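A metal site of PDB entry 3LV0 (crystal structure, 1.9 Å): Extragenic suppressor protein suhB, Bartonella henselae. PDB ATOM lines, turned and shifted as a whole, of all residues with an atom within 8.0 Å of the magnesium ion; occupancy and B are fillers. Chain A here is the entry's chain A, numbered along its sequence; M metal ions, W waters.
Water W1 lies within hydrogen-bond range of the side-chain hydroxyl of Thr 95 (2.7 Å) and the side-chain carboxylate of Glu 73 (3.3 Å). Water W2 lies within hydrogen-bond range of OE2 of Glu 74, OD1 of Asp 50 and N of Leu 92.
The side-chain carboxylate of Asp 50 lies within hydrogen-bond range of the side-chain hydroxyl of Thr 95 (2.6 Å). The side-chain carboxylate of Glu 74 is in salt-bridge range of the side-chain amino group of Lys 40 (2.8 Å). The backbone NH (N) of Glu 73 sits at hydrogen-bond distance from the backbone carbonyl oxygen (O) of Val 89. The backbone NH (N) of Ser 108 sits at hydrogen-bond distance from the backbone carbonyl oxygen (O) of Asp 90, 2.9 Å away. The backbone NH of Glu 74 is in hydrogen-bond range of the side-chain carboxylate of Glu 54 (2.7 Å). N of Asp 93 lies within hydrogen-bond range of O of Ala 106. The backbone NH (N) of Glu 73 sits at hydrogen-bond distance from the side-chain carboxylate (OE1) of Glu 54, 3.3 Å away. OG1 of Thr 95 sits close to O of Leu 92, at 3.4 Å.
Residues that only touch the magnesium ion: Asp 93 (3.95 Å), Thr 95 (3.99 Å) and Glu 74 (3.99 Å). The nearest printed residue that does not touch the magnesium ion is Asp 50 (4.2 Å).
OE1 of Glu 73 binds the magnesium ion (2.0 Å). O of Leu 92 is bound to the magnesium ion, 2.0 Å away. Water W2 binds the magnesium ion (2.0 Å). Water W1 binds the magnesium ion (2.1 Å). OD1 of Asp 90 is bound to the magnesium ion (2.1 Å). The magnesium ion is bound by water W3 (2.2 Å). The magnesium ion has six donor atoms within binding distance.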
ATOM      1  N   LYS A  40     -18.299   8.218  24.205  1.00  0.00           N
ATOM      2  CA  LYS A  40     -18.530   6.791  24.387  1.00  0.00           C
ATOM      3  C   LYS A  40     -17.856   6.336  25.688  1.00  0.00           C
ATOM      4  O   LYS A  40     -18.228   5.320  26.253  1.00  0.00           O
ATOM      5  CB  LYS A  40     -17.989   6.008  23.201  1.00  0.00           C
ATOM      6  CG  LYS A  40     -18.625   6.397  21.877  1.00  0.00           C
ATOM      7  CD  LYS A  40     -18.348   5.369  20.759  1.00  0.00           C
ATOM      8  CE  LYS A  40     -16.910   5.429  20.285  1.00  0.00           C
ATOM      9  NZ  LYS A  40     -16.628   4.461  19.185  1.00  0.00           N
ATOM     10  N   ASP A  44     -13.367   9.779  24.679  1.00  0.00           N
ATOM     11  CA  ASP A  44     -13.543   8.852  23.575  1.00  0.00           C
ATOM     12  C   ASP A  44     -14.806   9.274  22.836  1.00  0.00           C
ATOM     13  O   ASP A  44     -15.923   9.030  23.314  1.00  0.00           O
ATOM     14  CB  ASP A  44     -13.595   7.408  24.111  1.00  0.00           C
ATOM     15  CG  ASP A  44     -13.663   6.363  22.997  1.00  0.00           C
ATOM     16  OD1 ASP A  44     -13.450   6.672  21.815  1.00  0.00           O
ATOM     17  OD2 ASP A  44     -13.965   5.196  23.345  1.00  0.00           O
ATOM     18  N   TYR A  45     -14.612   9.983  21.713  1.00  0.00           N
ATOM     19  CA  TYR A  45     -15.671  10.710  21.012  1.00  0.00           C
ATOM     20  C   TYR A  45     -16.145   9.970  19.774  1.00  0.00           C
ATOM     21  O   TYR A  45     -15.390   9.238  19.150  1.00  0.00           O
ATOM     22  CB  TYR A  45     -15.172  12.115  20.607  1.00  0.00           C
ATOM     23  CG  TYR A  45     -14.728  12.954  21.787  1.00  0.00           C
ATOM     24  CD1 TYR A  45     -15.640  13.705  22.528  1.00  0.00           C
ATOM     25  CD2 TYR A  45     -13.380  12.966  22.183  1.00  0.00           C
ATOM     26  CE1 TYR A  45     -15.218  14.456  23.644  1.00  0.00           C
ATOM     27  CE2 TYR A  45     -12.956  13.708  23.284  1.00  0.00           C
ATOM     28  CZ  TYR A  45     -13.870  14.453  24.001  1.00  0.00           C
ATOM     29  OH  TYR A  45     -13.423  15.177  25.088  1.00  0.00           O
ATOM     30  N   VAL A  46     -17.420  10.168  19.443  1.00  0.00           N
ATOM     31  CA  VAL A  46     -17.946   9.789  18.141  1.00  0.00           C
ATOM     32  C   VAL A  46     -18.793  10.974  17.692  1.00  0.00           C
ATOM     33  O   VAL A  46     -19.454  11.630  18.525  1.00  0.00           O
ATOM     34  CB  VAL A  46     -18.802   8.482  18.194  1.00  0.00           C
ATOM     35  CG1 VAL A  46     -20.010   8.633  19.154  1.00  0.00           C
ATOM     36  CG2 VAL A  46     -19.286   8.074  16.779  1.00  0.00           C
ATOM     37  N   ASP A  50     -18.151  10.460  11.825  1.00  0.00           N
ATOM     38  CA  ASP A  50     -17.876   9.029  11.940  1.00  0.00           C
ATOM     39  C   ASP A  50     -19.062   8.205  11.457  1.00  0.00           C
ATOM     40  O   ASP A  50     -18.894   7.245  10.731  1.00  0.00           O
ATOM     41  CB  ASP A  50     -17.566   8.564  13.376  1.00  0.00           C
ATOM     42  CG  ASP A  50     -16.527   9.420  14.066  1.00  0.00           C
ATOM     43  OD1 ASP A  50     -15.430   8.876  14.347  1.00  0.00           O
ATOM     44  OD2 ASP A  50     -16.822  10.597  14.363  1.00  0.00           O
ATOM     45  N   GLU A  54     -19.356   5.725   8.194  1.00  0.00           N
ATOM     46  CA  GLU A  54     -19.637   4.317   8.378  1.00  0.00           C
ATOM     47  C   GLU A  54     -20.828   3.881   7.513  1.00  0.00           C
ATOM     48  O   GLU A  54     -20.800   2.764   6.941  1.00  0.00           O
ATOM     49  CB  GLU A  54     -19.924   3.994   9.859  1.00  0.00           C
ATOM     50  CG  GLU A  54     -19.664   2.514  10.152  1.00  0.00           C
ATOM     51  CD  GLU A  54     -19.645   2.209  11.642  1.00  0.00           C
ATOM     52  OE1 GLU A  54     -18.545   2.207  12.231  1.00  0.00           O
ATOM     53  OE2 GLU A  54     -20.736   1.941  12.193  1.00  0.00           O
ATOM     54  N   GLU A  73     -16.676   0.011  13.878  1.00  0.00           N
ATOM     55  CA  GLU A  73     -16.521   0.720  15.140  1.00  0.00           C
ATOM     56  C   GLU A  73     -17.839   1.242  15.749  1.00  0.00           C
ATOM     57  O   GLU A  73     -18.067   1.066  16.957  1.00  0.00           O
ATOM     58  CB  GLU A  73     -15.557   1.901  15.008  1.00  0.00           C
ATOM     59  CG  GLU A  73     -15.312   2.528  16.400  1.00  0.00           C
ATOM     60  CD  GLU A  73     -14.270   3.632  16.394  1.00  0.00           C
ATOM     61  OE1 GLU A  73     -13.780   4.018  15.317  1.00  0.00           O
ATOM     62  OE2 GLU A  73     -13.946   4.085  17.502  1.00  0.00           O
ATOM     63  N   GLU A  74     -18.683   1.852  14.924  1.00  0.00           N
ATOM     64  CA  GLU A  74     -19.783   2.673  15.454  1.00  0.00           C
ATOM     65  C   GLU A  74     -21.143   1.994  15.444  1.00  0.00           C
ATOM     66  O   GLU A  74     -22.164   2.652  15.683  1.00  0.00           O
ATOM     67  CB  GLU A  74     -19.872   4.031  14.741  1.00  0.00           C
ATOM     68  CG  GLU A  74     -18.518   4.795  14.603  1.00  0.00           C
ATOM     69  CD  GLU A  74     -17.786   5.123  15.916  1.00  0.00           C
ATOM     70  OE1 GLU A  74     -18.362   4.909  17.012  1.00  0.00           O
ATOM     71  OE2 GLU A  74     -16.633   5.627  15.842  1.00  0.00           O
ATOM     72  N   VAL A  89     -14.069  -2.354   9.880  1.00  0.00           N
ATOM     73  CA  VAL A  89     -14.135  -0.956   9.492  1.00  0.00           C
ATOM     74  C   VAL A  89     -13.948   0.032  10.656  1.00  0.00           C
ATOM     75  O   VAL A  89     -14.694   0.004  11.651  1.00  0.00           O
ATOM     76  CB  VAL A  89     -15.514  -0.631   8.818  1.00  0.00           C
ATOM     77  CG1 VAL A  89     -15.561   0.828   8.355  1.00  0.00           C
ATOM     78  CG2 VAL A  89     -15.811  -1.559   7.623  1.00  0.00           C
ATOM     79  N   ASP A  90     -12.952   0.921  10.496  1.00  0.00           N
ATOM     80  CA  ASP A  90     -12.864   2.139  11.282  1.00  0.00           C
ATOM     81  C   ASP A  90     -13.215   3.275  10.322  1.00  0.00           C
ATOM     82  O   ASP A  90     -12.424   3.603   9.443  1.00  0.00           O
ATOM     83  CB  ASP A  90     -11.434   2.349  11.847  1.00  0.00           C
ATOM     84  CG  ASP A  90     -11.345   3.521  12.817  1.00  0.00           C
ATOM     85  OD1 ASP A  90     -12.338   4.264  13.007  1.00  0.00           O
ATOM     86  OD2 ASP A  90     -10.257   3.706  13.427  1.00  0.00           O
ATOM     87  N   PRO A  91     -14.402   3.883  10.481  1.00  0.00           N
ATOM     88  CA  PRO A  91     -14.885   4.835   9.508  1.00  0.00           C
ATOM     89  C   PRO A  91     -14.173   6.152   9.709  1.00  0.00           C
ATOM     90  O   PRO A  91     -14.160   6.980   8.809  1.00  0.00           O
ATOM     91  CB  PRO A  91     -16.388   4.954   9.863  1.00  0.00           C
ATOM     92  CG  PRO A  91     -16.415   4.698  11.419  1.00  0.00           C
ATOM     93  CD  PRO A  91     -15.381   3.603  11.565  1.00  0.00           C
ATOM     94  N   LEU A  92     -13.566   6.347  10.889  1.00  0.00           N
ATOM     95  CA  LEU A  92     -12.763   7.526  11.112  1.00  0.00           C
ATOM     96  C   LEU A  92     -11.756   7.241  12.196  1.00  0.00           C
ATOM     97  O   LEU A  92     -12.093   7.079  13.381  1.00  0.00           O
ATOM     98  CB  LEU A  92     -13.633   8.734  11.477  1.00  0.00           C
ATOM     99  CG  LEU A  92     -12.960  10.084  11.823  1.00  0.00           C
ATOM    100  CD1 LEU A  92     -11.864  10.499  10.876  1.00  0.00           C
ATOM    101  CD2 LEU A  92     -14.062  11.152  12.025  1.00  0.00           C
ATOM    102  N   ASP A  93     -10.506   7.130  11.755  1.00  0.00           N
ATOM    103  CA  ASP A  93      -9.351   6.952  12.589  1.00  0.00           C
ATOM    104  C   ASP A  93      -8.805   8.346  12.851  1.00  0.00           C
ATOM    105  O   ASP A  93      -8.391   9.016  11.937  1.00  0.00           O
ATOM    106  CB  ASP A  93      -8.332   6.107  11.770  1.00  0.00           C
ATOM    107  CG  ASP A  93      -6.928   6.151  12.344  1.00  0.00           C
ATOM    108  OD1 ASP A  93      -6.785   5.997  13.574  1.00  0.00           O
ATOM    109  OD2 ASP A  93      -5.966   6.318  11.552  1.00  0.00           O
ATOM    110  N   GLY A  94      -8.834   8.770  14.107  1.00  0.00           N
ATOM    111  CA  GLY A  94      -8.473  10.140  14.481  1.00  0.00           C
ATOM    112  C   GLY A  94      -9.637  11.080  14.684  1.00  0.00           C
ATOM    113  O   GLY A  94      -9.604  12.246  14.275  1.00  0.00           O
ATOM    114  N   THR A  95     -10.686  10.600  15.350  1.00  0.00           N
ATOM    115  CA  THR A  95     -11.871  11.428  15.613  1.00  0.00           C
ATOM    116  C   THR A  95     -11.540  12.686  16.427  1.00  0.00           C
ATOM    117  O   THR A  95     -12.017  13.764  16.113  1.00  0.00           O
ATOM    118  CB  THR A  95     -12.937  10.582  16.344  1.00  0.00           C
ATOM    119  OG1 THR A  95     -13.218   9.458  15.523  1.00  0.00           O
ATOM    120  CG2 THR A  95     -14.250  11.400  16.582  1.00  0.00           C
ATOM    121  N   THR A  96     -10.753  12.548  17.480  1.00  0.00           N
ATOM    122  CA  THR A  96     -10.367  13.753  18.224  1.00  0.00           C
ATOM    123  C   THR A  96      -9.653  14.788  17.290  1.00  0.00           C
ATOM    124  O   THR A  96      -9.992  15.961  17.291  1.00  0.00           O
ATOM    125  CB  THR A  96      -9.526  13.367  19.444  1.00  0.00           C
ATOM    126  OG1 THR A  96     -10.350  12.585  20.310  1.00  0.00           O
ATOM    127  CG2 THR A  96      -9.000  14.646  20.196  1.00  0.00           C
ATOM    128  N   ALA A 106      -8.013   9.213   9.053  1.00  0.00           N
ATOM    129  CA  ALA A 106      -8.089   8.280   7.946  1.00  0.00           C
ATOM    130  C   ALA A 106      -9.350   7.431   8.046  1.00  0.00           C
ATOM    131  O   ALA A 106     -10.003   7.354   9.103  1.00  0.00           O
ATOM    132  CB  ALA A 106      -6.837   7.339   7.910  1.00  0.00           C
ATOM    133  N   VAL A 107      -9.660   6.778   6.933  1.00  0.00           N
ATOM    134  CA  VAL A 107     -10.650   5.717   6.947  1.00  0.00           C
ATOM    135  C   VAL A 107      -9.841   4.441   6.847  1.00  0.00           C
ATOM    136  O   VAL A 107      -8.870   4.400   6.095  1.00  0.00           O
ATOM    137  CB  VAL A 107     -11.566   5.857   5.684  1.00  0.00           C
ATOM    138  CG1 VAL A 107     -12.504   4.647   5.565  1.00  0.00           C
ATOM    139  CG2 VAL A 107     -12.350   7.189   5.726  1.00  0.00           C
ATOM    140  N   SER A 108     -10.243   3.385   7.576  1.00  0.00           N
ATOM    141  CA  SER A 108      -9.522   2.097   7.493  1.00  0.00           C
ATOM    142  C   SER A 108     -10.520   0.982   7.225  1.00  0.00           C
ATOM    143  O   SER A 108     -11.517   0.862   7.957  1.00  0.00           O
ATOM    144  CB  SER A 108      -8.796   1.821   8.834  1.00  0.00           C
ATOM    145  OG  SER A 108      -8.071   0.600   8.737  1.00  0.00           O
ATOM    146  N   TRP A 217     -10.445  -2.822  14.753  1.00  0.00           N
ATOM    147  CA  TRP A 217     -10.620  -1.918  13.611  1.00  0.00           C
ATOM    148  C   TRP A 217      -9.506  -0.887  13.489  1.00  0.00           C
ATOM    149  O   TRP A 217      -9.244  -0.375  12.400  1.00  0.00           O
ATOM    150  CB  TRP A 217     -11.993  -1.240  13.614  1.00  0.00           C
ATOM    151  CG  TRP A 217     -12.368  -0.676  14.915  1.00  0.00           C
ATOM    152  CD1 TRP A 217     -11.892   0.481  15.490  1.00  0.00           C
ATOM    153  CD2 TRP A 217     -13.300  -1.229  15.839  1.00  0.00           C
ATOM    154  NE1 TRP A 217     -12.483   0.674  16.724  1.00  0.00           N
ATOM    155  CE2 TRP A 217     -13.352  -0.368  16.967  1.00  0.00           C
ATOM    156  CE3 TRP A 217     -14.094  -2.377  15.844  1.00  0.00           C
ATOM    157  CZ2 TRP A 217     -14.183  -0.613  18.077  1.00  0.00           C
ATOM    158  CZ3 TRP A 217     -14.929  -2.631  16.951  1.00  0.00           C
ATOM    159  CH2 TRP A 217     -14.961  -1.740  18.050  1.00  0.00           C
ATOM    160  N   ASP A 218      -8.837  -0.597  14.612  1.00  0.00           N
ATOM    161  CA  ASP A 218      -7.732   0.365  14.593  1.00  0.00           C
ATOM    162  C   ASP A 218      -6.557  -0.222  13.813  1.00  0.00           C
ATOM    163  O   ASP A 218      -5.876   0.501  13.100  1.00  0.00           O
ATOM    164  CB  ASP A 218      -7.251   0.673  16.021  1.00  0.00           C
ATOM    165  CG  ASP A 218      -8.276   1.478  16.830  1.00  0.00           C
ATOM    166  OD1 ASP A 218      -8.777   2.478  16.288  1.00  0.00           O
ATOM    167  OD2 ASP A 218      -8.542   1.108  17.988  1.00  0.00           O
HETATM  168 MG    MG M   1     -12.865   5.611  14.538  1.00  0.00          MG
HETATM  169  O   HOH W   1     -12.894   6.897  16.152  1.00  0.00           O
HETATM  170  O   HOH W   2     -14.764   6.159  14.074  1.00  0.00           O
HETATM  171  O   HOH W   3     -10.908   5.140  15.406  1.00  0.00           O
